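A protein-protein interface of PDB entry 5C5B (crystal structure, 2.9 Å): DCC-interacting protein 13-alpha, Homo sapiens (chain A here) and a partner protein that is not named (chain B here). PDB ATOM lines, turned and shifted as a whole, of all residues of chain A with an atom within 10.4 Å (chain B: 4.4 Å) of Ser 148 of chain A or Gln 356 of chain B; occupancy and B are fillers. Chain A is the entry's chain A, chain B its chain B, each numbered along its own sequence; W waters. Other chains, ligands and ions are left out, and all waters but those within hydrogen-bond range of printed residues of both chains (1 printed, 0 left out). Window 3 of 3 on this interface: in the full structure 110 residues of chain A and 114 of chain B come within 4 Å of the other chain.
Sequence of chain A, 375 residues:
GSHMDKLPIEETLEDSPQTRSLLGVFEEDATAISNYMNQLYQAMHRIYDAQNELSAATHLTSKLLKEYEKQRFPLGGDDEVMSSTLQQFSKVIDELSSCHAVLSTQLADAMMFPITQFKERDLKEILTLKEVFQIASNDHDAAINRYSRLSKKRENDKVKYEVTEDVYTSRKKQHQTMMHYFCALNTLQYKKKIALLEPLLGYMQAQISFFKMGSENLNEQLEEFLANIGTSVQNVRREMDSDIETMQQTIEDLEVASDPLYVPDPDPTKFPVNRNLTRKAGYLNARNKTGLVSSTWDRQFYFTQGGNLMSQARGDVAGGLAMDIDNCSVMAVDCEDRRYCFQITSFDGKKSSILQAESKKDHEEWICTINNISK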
ATOM      1  N   HIS A 140     -32.671  -1.419  21.429  1.00  0.00           N
ATOM      2  CA  HIS A 140     -31.265  -1.066  21.256  1.00  0.00           C
ATOM      3  C   HIS A 140     -30.543  -0.963  22.594  1.00  0.00           C
ATOM      4  O   HIS A 140     -29.388  -1.381  22.716  1.00  0.00           O
ATOM      5  CB  HIS A 140     -31.108   0.249  20.496  1.00  0.00           C
ATOM      6  CG  HIS A 140     -29.683   0.680  20.344  1.00  0.00           C
ATOM      7  ND1 HIS A 140     -29.139   1.721  21.065  1.00  0.00           N
ATOM      8  CD2 HIS A 140     -28.680   0.191  19.575  1.00  0.00           C
ATOM      9  CE1 HIS A 140     -27.868   1.865  20.736  1.00  0.00           C
ATOM     10  NE2 HIS A 140     -27.565   0.950  19.834  1.00  0.00           N
ATOM     11  N   ASP A 141     -31.223  -0.396  23.586  1.00  0.00           N
ATOM     12  CA  ASP A 141     -30.661  -0.283  24.927  1.00  0.00           C
ATOM     13  C   ASP A 141     -30.269  -1.665  25.436  1.00  0.00           C
ATOM     14  O   ASP A 141     -29.117  -1.898  25.830  1.00  0.00           O
ATOM     15  CB  ASP A 141     -31.662   0.373  25.883  1.00  0.00           C
ATOM     16  CG  ASP A 141     -31.937   1.825  25.536  1.00  0.00           C
ATOM     17  OD1 ASP A 141     -31.073   2.464  24.900  1.00  0.00           O
ATOM     18  OD2 ASP A 141     -33.022   2.327  25.902  1.00  0.00           O
ATOM     19  N   ALA A 142     -31.235  -2.581  25.404  1.00  0.00           N
ATOM     20  CA  ALA A 142     -30.991  -3.968  25.793  1.00  0.00           C
ATOM     21  C   ALA A 142     -29.800  -4.568  25.037  1.00  0.00           C
ATOM     22  O   ALA A 142     -28.897  -5.167  25.640  1.00  0.00           O
ATOM     23  CB  ALA A 142     -32.240  -4.802  25.560  1.00  0.00           C
ATOM     24  N   ALA A 143     -29.803  -4.387  23.719  1.00  0.00           N
ATOM     25  CA  ALA A 143     -28.775  -4.960  22.854  1.00  0.00           C
ATOM     26  C   ALA A 143     -27.368  -4.495  23.229  1.00  0.00           C
ATOM     27  O   ALA A 143     -26.459  -5.315  23.403  1.00  0.00           O
ATOM     28  CB  ALA A 143     -29.069  -4.622  21.400  1.00  0.00           C
ATOM     29  N   ILE A 144     -27.192  -3.185  23.371  1.00  0.00           N
ATOM     30  CA  ILE A 144     -25.872  -2.646  23.679  1.00  0.00           C
ATOM     31  C   ILE A 144     -25.470  -2.964  25.119  1.00  0.00           C
ATOM     32  O   ILE A 144     -24.281  -3.024  25.431  1.00  0.00           O
ATOM     33  CB  ILE A 144     -25.798  -1.117  23.438  1.00  0.00           C
ATOM     34  CG1 ILE A 144     -24.339  -0.662  23.331  1.00  0.00           C
ATOM     35  CG2 ILE A 144     -26.534  -0.350  24.527  1.00  0.00           C
ATOM     36  N   ASN A 145     -26.449  -3.183  25.997  1.00  0.00           N
ATOM     37  CA  ASN A 145     -26.116  -3.621  27.351  1.00  0.00           C
ATOM     38  C   ASN A 145     -25.561  -5.043  27.347  1.00  0.00           C
ATOM     39  O   ASN A 145     -24.561  -5.337  28.020  1.00  0.00           O
ATOM     40  CB  ASN A 145     -27.336  -3.527  28.270  1.00  0.00           C
ATOM     41  CG  ASN A 145     -27.758  -2.095  28.530  1.00  0.00           C
ATOM     42  OD1 ASN A 145     -26.934  -1.180  28.504  1.00  0.00           O
ATOM     43  ND2 ASN A 145     -29.046  -1.894  28.784  1.00  0.00           N
ATOM     44  N   ARG A 146     -26.185  -5.918  26.561  1.00  0.00           N
ATOM     45  CA  ARG A 146     -25.691  -7.286  26.450  1.00  0.00           C
ATOM     46  C   ARG A 146     -24.351  -7.304  25.721  1.00  0.00           C
ATOM     47  O   ARG A 146     -23.541  -8.209  25.923  1.00  0.00           O
ATOM     48  CB  ARG A 146     -26.704  -8.191  25.743  1.00  0.00           C
ATOM     49  CG  ARG A 146     -27.332  -9.228  26.666  1.00  0.00           C
ATOM     50  CD  ARG A 146     -28.818  -9.418  26.403  1.00  0.00           C
ATOM     51  NE  ARG A 146     -29.408 -10.383  27.329  1.00  0.00           N
ATOM     52  CZ  ARG A 146     -30.621 -10.910  27.196  1.00  0.00           C
ATOM     53  NH1 ARG A 146     -31.069 -11.780  28.091  1.00  0.00           N
ATOM     54  NH2 ARG A 146     -31.387 -10.566  26.169  1.00  0.00           N
ATOM     55  N   TYR A 147     -24.124  -6.308  24.868  1.00  0.00           N
ATOM     56  CA  TYR A 147     -22.834  -6.171  24.198  1.00  0.00           C
ATOM     57  C   TYR A 147     -21.751  -5.767  25.190  1.00  0.00           C
ATOM     58  O   TYR A 147     -20.636  -6.291  25.161  1.00  0.00           O
ATOM     59  CB  TYR A 147     -22.913  -5.150  23.066  1.00  0.00           C
ATOM     60  CG  TYR A 147     -21.613  -4.990  22.309  1.00  0.00           C
ATOM     61  CD1 TYR A 147     -21.253  -5.888  21.314  1.00  0.00           C
ATOM     62  CD2 TYR A 147     -20.747  -3.941  22.590  1.00  0.00           C
ATOM     63  CE1 TYR A 147     -20.066  -5.745  20.619  1.00  0.00           C
ATOM     64  CE2 TYR A 147     -19.560  -3.790  21.903  1.00  0.00           C
ATOM     65  CZ  TYR A 147     -19.224  -4.695  20.918  1.00  0.00           C
ATOM     66  OH  TYR A 147     -18.039  -4.547  20.231  1.00  0.00           O
ATOM     67  N   SER A 148     -22.084  -4.817  26.058  1.00  0.00           N
ATOM     68  CA  SER A 148     -21.170  -4.375  27.100  1.00  0.00           C
ATOM     69  C   SER A 148     -20.820  -5.513  28.050  1.00  0.00           C
ATOM     70  O   SER A 148     -19.685  -5.612  28.518  1.00  0.00           O
ATOM     71  CB  SER A 148     -21.774  -3.209  27.882  1.00  0.00           C
ATOM     72  OG  SER A 148     -21.958  -2.080  27.047  1.00  0.00           O
ATOM     73  N   ARG A 149     -21.796  -6.369  28.334  1.00  0.00           N
ATOM     74  CA  ARG A 149     -21.584  -7.466  29.277  1.00  0.00           C
ATOM     75  C   ARG A 149     -20.713  -8.606  28.741  1.00  0.00           C
ATOM     76  O   ARG A 149     -20.397  -9.535  29.482  1.00  0.00           O
ATOM     77  CB  ARG A 149     -22.925  -8.027  29.745  1.00  0.00           C
ATOM     78  CG  ARG A 149     -23.538  -7.230  30.882  1.00  0.00           C
ATOM     79  CD  ARG A 149     -24.824  -7.857  31.382  1.00  0.00           C
ATOM     80  NE  ARG A 149     -25.415  -7.079  32.466  1.00  0.00           N
ATOM     81  N   LEU A 150     -20.342  -8.549  27.464  1.00  0.00           N
ATOM     82  CA  LEU A 150     -19.460  -9.559  26.876  1.00  0.00           C
ATOM     83  C   LEU A 150     -18.172  -9.741  27.687  1.00  0.00           C
ATOM     84  O   LEU A 150     -17.612  -8.772  28.196  1.00  0.00           O
ATOM     85  CB  LEU A 150     -19.106  -9.189  25.433  1.00  0.00           C
ATOM     86  CG  LEU A 150     -20.120  -9.501  24.327  1.00  0.00           C
ATOM     87  CD1 LEU A 150     -19.532  -9.199  22.954  1.00  0.00           C
ATOM     88  CD2 LEU A 150     -20.582 -10.945  24.402  1.00  0.00           C
ATOM     89  N   SER A 151     -17.706 -10.984  27.785  1.00  0.00           N
ATOM     90  CA  SER A 151     -16.498 -11.322  28.542  1.00  0.00           C
ATOM     91  C   SER A 151     -15.233 -11.059  27.735  1.00  0.00           C
ATOM     92  O   SER A 151     -15.146 -11.457  26.582  1.00  0.00           O
ATOM     93  CB  SER A 151     -16.546 -12.786  28.968  1.00  0.00           C
ATOM     94  OG  SER A 151     -15.297 -13.216  29.479  1.00  0.00           O
ATOM     95  N   LYS A 152     -14.245 -10.407  28.341  1.00  0.00           N
ATOM     96  CA  LYS A 152     -13.037 -10.042  27.600  1.00  0.00           C
ATOM     97  C   LYS A 152     -12.034 -11.175  27.341  1.00  0.00           C
ATOM     98  O   LYS A 152     -11.612 -11.369  26.202  1.00  0.00           O
ATOM     99  CB  LYS A 152     -12.310  -8.892  28.303  1.00  0.00           C
ATOM    100  CG  LYS A 152     -11.049  -8.458  27.559  1.00  0.00           C
ATOM    101  CD  LYS A 152     -10.041  -7.780  28.474  1.00  0.00           C
ATOM    102  CE  LYS A 152      -9.188  -6.770  27.714  1.00  0.00           C
ATOM    103  NZ  LYS A 152      -8.090  -6.212  28.559  1.00  0.00           N
ATOM    104  N   LYS A 153     -11.641 -11.913  28.375  1.00  0.00           N
ATOM    105  CA  LYS A 153     -10.511 -12.832  28.234  1.00  0.00           C
ATOM    106  C   LYS A 153     -10.912 -14.172  27.614  1.00  0.00           C
ATOM    107  O   LYS A 153     -10.155 -14.757  26.838  1.00  0.00           O
ATOM    108  CB  LYS A 153      -9.828 -13.051  29.588  1.00  0.00           C
ATOM    109  CG  LYS A 153     -10.533 -14.029  30.517  1.00  0.00           C
ATOM    110  CD  LYS A 153      -9.714 -14.298  31.765  1.00  0.00           C
ATOM    111  CE  LYS A 153      -8.871 -13.096  32.145  1.00  0.00           C
ATOM    112  NZ  LYS A 153      -7.889 -13.449  33.199  1.00  0.00           N
ATOM    113  N   GLU A 155     -13.456 -15.374  25.082  1.00  0.00           N
ATOM    114  CA  GLU A 155     -14.462 -15.004  24.108  1.00  0.00           C
ATOM    115  C   GLU A 155     -14.867 -16.143  23.188  1.00  0.00           C
ATOM    116  O   GLU A 155     -14.037 -16.777  22.535  1.00  0.00           O
ATOM    117  CB  GLU A 155     -13.973 -13.801  23.303  1.00  0.00           C
ATOM    118  CG  GLU A 155     -14.584 -12.492  23.786  1.00  0.00           C
ATOM    119  CD  GLU A 155     -13.681 -11.286  23.588  1.00  0.00           C
ATOM    120  OE1 GLU A 155     -12.982 -11.220  22.556  1.00  0.00           O
ATOM    121  OE2 GLU A 155     -13.699 -10.381  24.448  1.00  0.00           O
ATOM    122  N   VAL A 159     -21.398 -16.501  20.327  1.00  0.00           N
ATOM    123  CA  VAL A 159     -22.238 -15.640  21.157  1.00  0.00           C
ATOM    124  C   VAL A 159     -21.882 -14.166  20.950  1.00  0.00           C
ATOM    125  O   VAL A 159     -22.764 -13.304  20.908  1.00  0.00           O
ATOM    126  CB  VAL A 159     -22.139 -16.016  22.664  1.00  0.00           C
ATOM    127  CG1 VAL A 159     -20.719 -15.868  23.191  1.00  0.00           C
ATOM    128  CG2 VAL A 159     -23.119 -15.193  23.491  1.00  0.00           C
ATOM    129  N   LYS A 160     -20.590 -13.889  20.793  1.00  0.00           N
ATOM    130  CA  LYS A 160     -20.112 -12.531  20.570  1.00  0.00           C
ATOM    131  C   LYS A 160     -20.674 -11.956  19.276  1.00  0.00           C
ATOM    132  O   LYS A 160     -21.125 -10.814  19.242  1.00  0.00           O
ATOM    133  CB  LYS A 160     -18.583 -12.500  20.539  1.00  0.00           C
ATOM    134  CG  LYS A 160     -18.001 -11.217  19.973  1.00  0.00           C
ATOM    135  CD  LYS A 160     -16.491 -11.302  19.863  1.00  0.00           C
ATOM    136  CE  LYS A 160     -15.898  -9.985  19.396  1.00  0.00           C
ATOM    137  NZ  LYS A 160     -14.416 -10.056  19.290  1.00  0.00           N
ATOM    138  N   VAL A 163     -24.550 -11.387  19.599  1.00  0.00           N
ATOM    139  CA  VAL A 163     -24.809 -10.172  20.362  1.00  0.00           C
ATOM    140  C   VAL A 163     -24.464  -8.925  19.547  1.00  0.00           C
ATOM    141  O   VAL A 163     -25.230  -7.952  19.515  1.00  0.00           O
ATOM    142  CB  VAL A 163     -24.011 -10.152  21.682  1.00  0.00           C
ATOM    143  CG1 VAL A 163     -24.161  -8.814  22.361  1.00  0.00           C
ATOM    144  CG2 VAL A 163     -24.479 -11.263  22.606  1.00  0.00           C
ATOM    145  N   THR A 164     -23.321  -8.972  18.871  1.00  0.00           N
ATOM    146  CA  THR A 164     -22.864  -7.863  18.041  1.00  0.00           C
ATOM    147  C   THR A 164     -23.858  -7.466  16.955  1.00  0.00           C
ATOM    148  O   THR A 164     -24.149  -6.283  16.777  1.00  0.00           O
ATOM    149  CB  THR A 164     -21.523  -8.202  17.353  1.00  0.00           C
ATOM    150  OG1 THR A 164     -20.558  -8.590  18.338  1.00  0.00           O
ATOM    151  CG2 THR A 164     -21.002  -7.004  16.576  1.00  0.00           C
ATOM    152  N   VAL A 167     -26.987  -6.018  18.193  1.00  0.00           N
ATOM    153  CA  VAL A 167     -26.732  -4.596  18.391  1.00  0.00           C
ATOM    154  C   VAL A 167     -26.868  -3.864  17.064  1.00  0.00           C
ATOM    155  O   VAL A 167     -27.491  -2.806  16.991  1.00  0.00           O
ATOM    156  CB  VAL A 167     -25.332  -4.340  18.983  1.00  0.00           C
ATOM    157  CG1 VAL A 167     -24.964  -2.862  18.888  1.00  0.00           C
ATOM    158  CG2 VAL A 167     -25.271  -4.824  20.416  1.00  0.00           C
ATOM    159  N   ARG A 171     -29.792  -1.139  16.460  1.00  0.00           N
ATOM    160  CA  ARG A 171     -29.274   0.201  16.205  1.00  0.00           C
ATOM    161  C   ARG A 171     -29.790   0.744  14.879  1.00  0.00           C
ATOM    162  O   ARG A 171     -30.226   1.898  14.795  1.00  0.00           O
ATOM    163  CB  ARG A 171     -27.743   0.196  16.205  1.00  0.00           C
ATOM    164  CG  ARG A 171     -27.113   1.579  16.166  1.00  0.00           C
ATOM    165  CD  ARG A 171     -25.621   1.523  16.462  1.00  0.00           C
ATOM    166  NE  ARG A 171     -25.342   1.183  17.853  1.00  0.00           N
ATOM    167  CZ  ARG A 171     -24.122   1.008  18.349  1.00  0.00           C
ATOM    168  NH1 ARG A 171     -23.059   1.143  17.566  1.00  0.00           N
ATOM    169  NH2 ARG A 171     -23.961   0.700  19.629  1.00  0.00           N
ATOM    170  N   LEU B 284     -20.622   6.375  26.675  1.00  0.00           N
ATOM    171  CA  LEU B 284     -19.722   5.498  27.409  1.00  0.00           C
ATOM    172  C   LEU B 284     -20.461   4.875  28.581  1.00  0.00           C
ATOM    173  O   LEU B 284     -21.497   5.382  29.012  1.00  0.00           O
ATOM    174  CB  LEU B 284     -18.496   6.262  27.908  1.00  0.00           C
ATOM    175  CG  LEU B 284     -17.536   6.846  26.871  1.00  0.00           C
ATOM    176  CD1 LEU B 284     -16.472   7.684  27.560  1.00  0.00           C
ATOM    177  CD2 LEU B 284     -16.897   5.745  26.040  1.00  0.00           C
ATOM    178  N   ASN B 285     -19.931   3.774  29.095  1.00  0.00           N
ATOM    179  CA  ASN B 285     -20.492   3.178  30.294  1.00  0.00           C
ATOM    180  C   ASN B 285     -19.687   3.584  31.517  1.00  0.00           C
ATOM    181  O   ASN B 285     -18.500   3.276  31.625  1.00  0.00           O
ATOM    182  CB  ASN B 285     -20.546   1.656  30.171  1.00  0.00           C
ATOM    183  CG  ASN B 285     -21.587   1.192  29.172  1.00  0.00           C
ATOM    184  OD1 ASN B 285     -22.604   1.854  28.963  1.00  0.00           O
ATOM    185  ND2 ASN B 285     -21.337   0.048  28.547  1.00  0.00           N
ATOM    186  N   TRP B 297     -23.190  -0.363  36.160  1.00  0.00           N
ATOM    187  CA  TRP B 297     -22.720   0.375  34.994  1.00  0.00           C
ATOM    188  C   TRP B 297     -23.879   1.165  34.398  1.00  0.00           C
ATOM    189  O   TRP B 297     -24.999   0.664  34.311  1.00  0.00           O
ATOM    190  CB  TRP B 297     -22.117  -0.567  33.947  1.00  0.00           C
ATOM    191  CG  TRP B 297     -20.878  -1.288  34.406  1.00  0.00           C
ATOM    192  CD1 TRP B 297     -20.821  -2.413  35.175  1.00  0.00           C
ATOM    193  CD2 TRP B 297     -19.516  -0.931  34.115  1.00  0.00           C
ATOM    194  NE1 TRP B 297     -19.512  -2.778  35.383  1.00  0.00           N
ATOM    195  CE2 TRP B 297     -18.696  -1.890  34.745  1.00  0.00           C
ATOM    196  CE3 TRP B 297     -18.919   0.101  33.388  1.00  0.00           C
ATOM    197  CZ2 TRP B 297     -17.303  -1.840  34.665  1.00  0.00           C
ATOM    198  CZ3 TRP B 297     -17.538   0.145  33.311  1.00  0.00           C
ATOM    199  CH2 TRP B 297     -16.745  -0.819  33.947  1.00  0.00           C
ATOM    200  N   ARG B 338     -14.601  -7.030  31.269  1.00  0.00           N
ATOM    201  CA  ARG B 338     -15.310  -6.237  30.272  1.00  0.00           C
ATOM    202  C   ARG B 338     -14.353  -5.719  29.207  1.00  0.00           C
ATOM    203  O   ARG B 338     -13.189  -5.432  29.488  1.00  0.00           O
ATOM    204  CB  ARG B 338     -16.041  -5.068  30.933  1.00  0.00           C
ATOM    205  CG  ARG B 338     -17.466  -5.381  31.353  1.00  0.00           C
ATOM    206  CD  ARG B 338     -18.107  -4.187  32.039  1.00  0.00           C
ATOM    207  NE  ARG B 338     -19.366  -4.537  32.691  1.00  0.00           N
ATOM    208  CZ  ARG B 338     -20.564  -4.158  32.257  1.00  0.00           C
ATOM    209  NH1 ARG B 338     -20.669  -3.409  31.168  1.00  0.00           N
ATOM    210  NH2 ARG B 338     -21.655  -4.525  32.913  1.00  0.00           N
ATOM    211  N   ARG B 339     -14.853  -5.611  27.982  1.00  0.00           N
ATOM    212  CA  ARG B 339     -14.039  -5.170  26.859  1.00  0.00           C
ATOM    213  C   ARG B 339     -13.980  -3.648  26.775  1.00  0.00           C
ATOM    214  O   ARG B 339     -14.977  -2.965  27.012  1.00  0.00           O
ATOM    215  CB  ARG B 339     -14.587  -5.740  25.550  1.00  0.00           C
ATOM    216  CG  ARG B 339     -14.375  -7.230  25.386  1.00  0.00           C
ATOM    217  CD  ARG B 339     -15.369  -7.818  24.398  1.00  0.00           C
ATOM    218  NE  ARG B 339     -15.046  -7.477  23.016  1.00  0.00           N
ATOM    219  CZ  ARG B 339     -15.798  -6.695  22.249  1.00  0.00           C
ATOM    220  NH1 ARG B 339     -16.917  -6.174  22.734  1.00  0.00           N
ATOM    221  NH2 ARG B 339     -15.434  -6.435  21.001  1.00  0.00           N
ATOM    222  N   TYR B 340     -12.793  -3.135  26.458  1.00  0.00           N
ATOM    223  CA  TYR B 340     -12.587  -1.721  26.143  1.00  0.00           C
ATOM    224  C   TYR B 340     -12.886  -0.787  27.310  1.00  0.00           C
ATOM    225  O   TYR B 340     -13.534   0.246  27.139  1.00  0.00           O
ATOM    226  CB  TYR B 340     -13.434  -1.328  24.930  1.00  0.00           C
ATOM    227  CG  TYR B 340     -13.155  -2.182  23.717  1.00  0.00           C
ATOM    228  CD1 TYR B 340     -11.851  -2.450  23.322  1.00  0.00           C
ATOM    229  CD2 TYR B 340     -14.192  -2.731  22.976  1.00  0.00           C
ATOM    230  CE1 TYR B 340     -11.589  -3.234  22.218  1.00  0.00           C
ATOM    231  CE2 TYR B 340     -13.937  -3.517  21.869  1.00  0.00           C
ATOM    232  CZ  TYR B 340     -12.635  -3.765  21.494  1.00  0.00           C
ATOM    233  OH  TYR B 340     -12.374  -4.548  20.392  1.00  0.00           O
ATOM    234  N   CYS B 341     -12.415  -1.155  28.495  1.00  0.00           N
ATOM    235  CA  CYS B 341     -12.465  -0.252  29.636  1.00  0.00           C
ATOM    236  C   CYS B 341     -11.180   0.562  29.734  1.00  0.00           C
ATOM    237  O   CYS B 341     -10.084   0.044  29.513  1.00  0.00           O
ATOM    238  CB  CYS B 341     -12.700  -1.028  30.934  1.00  0.00           C
ATOM    239  SG  CYS B 341     -14.321  -1.820  31.055  1.00  0.00           S
ATOM    240  N   LEU B 355     -14.381   3.947  32.779  1.00  0.00           N
ATOM    241  CA  LEU B 355     -15.323   4.070  31.675  1.00  0.00           C
ATOM    242  C   LEU B 355     -15.158   2.925  30.683  1.00  0.00           C
ATOM    243  O   LEU B 355     -14.122   2.265  30.654  1.00  0.00           O
ATOM    244  CB  LEU B 355     -15.136   5.407  30.960  1.00  0.00           C
ATOM    245  CG  LEU B 355     -15.402   6.650  31.803  1.00  0.00           C
ATOM    246  CD1 LEU B 355     -14.745   7.868  31.179  1.00  0.00           C
ATOM    247  CD2 LEU B 355     -16.894   6.858  31.946  1.00  0.00           C
ATOM    248  N   GLN B 356     -16.182   2.699  29.868  1.00  0.00           N
ATOM    249  CA  GLN B 356     -16.164   1.615  28.894  1.00  0.00           C
ATOM    250  C   GLN B 356     -16.679   2.069  27.533  1.00  0.00           C
ATOM    251  O   GLN B 356     -17.756   2.661  27.437  1.00  0.00           O
ATOM    252  CB  GLN B 356     -17.001   0.439  29.399  1.00  0.00           C
ATOM    253  CG  GLN B 356     -16.882  -0.822  28.565  1.00  0.00           C
ATOM    254  CD  GLN B 356     -17.998  -1.807  28.852  1.00  0.00           C
ATOM    255  OE1 GLN B 356     -18.905  -1.520  29.633  1.00  0.00           O
ATOM    256  NE2 GLN B 356     -17.937  -2.974  28.222  1.00  0.00           N
ATOM    257  N   ALA B 357     -15.910   1.793  26.482  1.00  0.00           N
ATOM    258  CA  ALA B 357     -16.366   2.076  25.126  1.00  0.00           C
ATOM    259  C   ALA B 357     -16.855   0.800  24.448  1.00  0.00           C
ATOM    260  O   ALA B 357     -16.706  -0.296  24.988  1.00  0.00           O
ATOM    261  CB  ALA B 357     -15.252   2.718  24.316  1.00  0.00           C
HETATM  262  O   HOH W   1     -17.124  -6.465  27.445  1.00  0.00           O
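The side-chain hydroxyl of Thr 164 of chain A lies within hydrogen-bond range of the backbone carbonyl oxygen of Lys 160 of chain A, 2.5 Å away.
The guanidinium group of Arg 338 of chain B is in hydrogen-bond range of the side-chain amide oxygen of Gln 356 of chain B (3.0 Å).
The side-chain hydroxyl of Ser 148 of chain A sits at hydrogen-bond distance from the backbone carbonyl oxygen of Ile 144 of chain A (3.0 Å).
N of Asn 285 of chain B is in hydrogen-bond range of O of Gln 356 of chain B (3.0 Å).
The side-chain carboxylate (OE1) of Glu 155 of chain A is in salt-bridge range of the side-chain amino group (NZ) of Lys 160 of chain A.
The backbone carbonyl oxygen (O) of Arg 339 of chain B sits at hydrogen-bond distance from the side-chain amide nitrogen (NE2) of Gln 356 of chain B.
Arg 338 of chain B touches Ser 148 of chain A.
Arg 149 of chain A touches Arg 338 of chain B (CG to NH2, 3.9 Å).
Arg 338 of chain B touches Lys 152 of chain A (O to CB, 3.8 Å).
Arg 339 of chain B touches Lys 152 of chain A (CG to CA, 3.8 Å).
Lys 160 of chain A touches Arg 339 of chain B.
Of the 10 printed residues of chain B, 4 touch a printed residue of chain A.
Along chain B the printed residues that touch a printed residue of chain A span positions 285 to 356.
Among the printed residues, Asp or Glu carboxylates within 4 Å of a Lys or Arg side-chain nitrogen of the other chain: Glu 155 of chain A with Arg 339 of chain B (3.5 Å).
Water W1 lies within hydrogen-bond range of the backbone carbonyl oxygen of Leu 150 of chain A (2.5 Å), the backbone NH of Arg 339 of chain B (2.5 Å) and the backbone carbonyl oxygen of Ser 148 of chain A (2.9 Å).
Of chain A, only Ser 148 (3.2 Å) comes within 4 Å of Gln 356 of chain B.
Leu 284 of chain B touches none of the printed residues of chain A.
Asn 285 of chain B touches just one residue of chain A: Ser 148 (2.7 Å).
No residue of chain A comes within 4 Å of Cys 341 of chain B.
Of the printed residues of chain A, Arg 338 of chain B touches Ser 148, Arg 149 and Lys 152.
Printed residues of chain B within 4 Å of Tyr 147 of chain A: Arg 339.
Of the printed residues of chain B, Glu 155 of chain A touches Arg 339.
Printed residues of chain B within 4 Å of Lys 160 of chain A: Arg 339 (3.9 Å).
Ala 142 of chain A touches none of the printed residues of chain B.
The side-chain carboxylate (OE2) of Glu 155 of chain A is in salt-bridge range of the guanidinium group (NE) of Arg 339 of chain B (3.5 Å).
The guanidinium group of Arg 339 of chain B sits at hydrogen-bond distance from the side-chain hydroxyl of Tyr 147 of chain A (3.2 Å).
The backbone carbonyl oxygen of Ser 148 of chain A lies within hydrogen-bond range of the side-chain amide nitrogen of Gln 356 of chain B, 3.2 Å away.
The side-chain amide nitrogen (ND2) of Asn 285 of chain B lies within hydrogen-bond range of the side-chain hydroxyl (OG) of Ser 148 of chain A.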
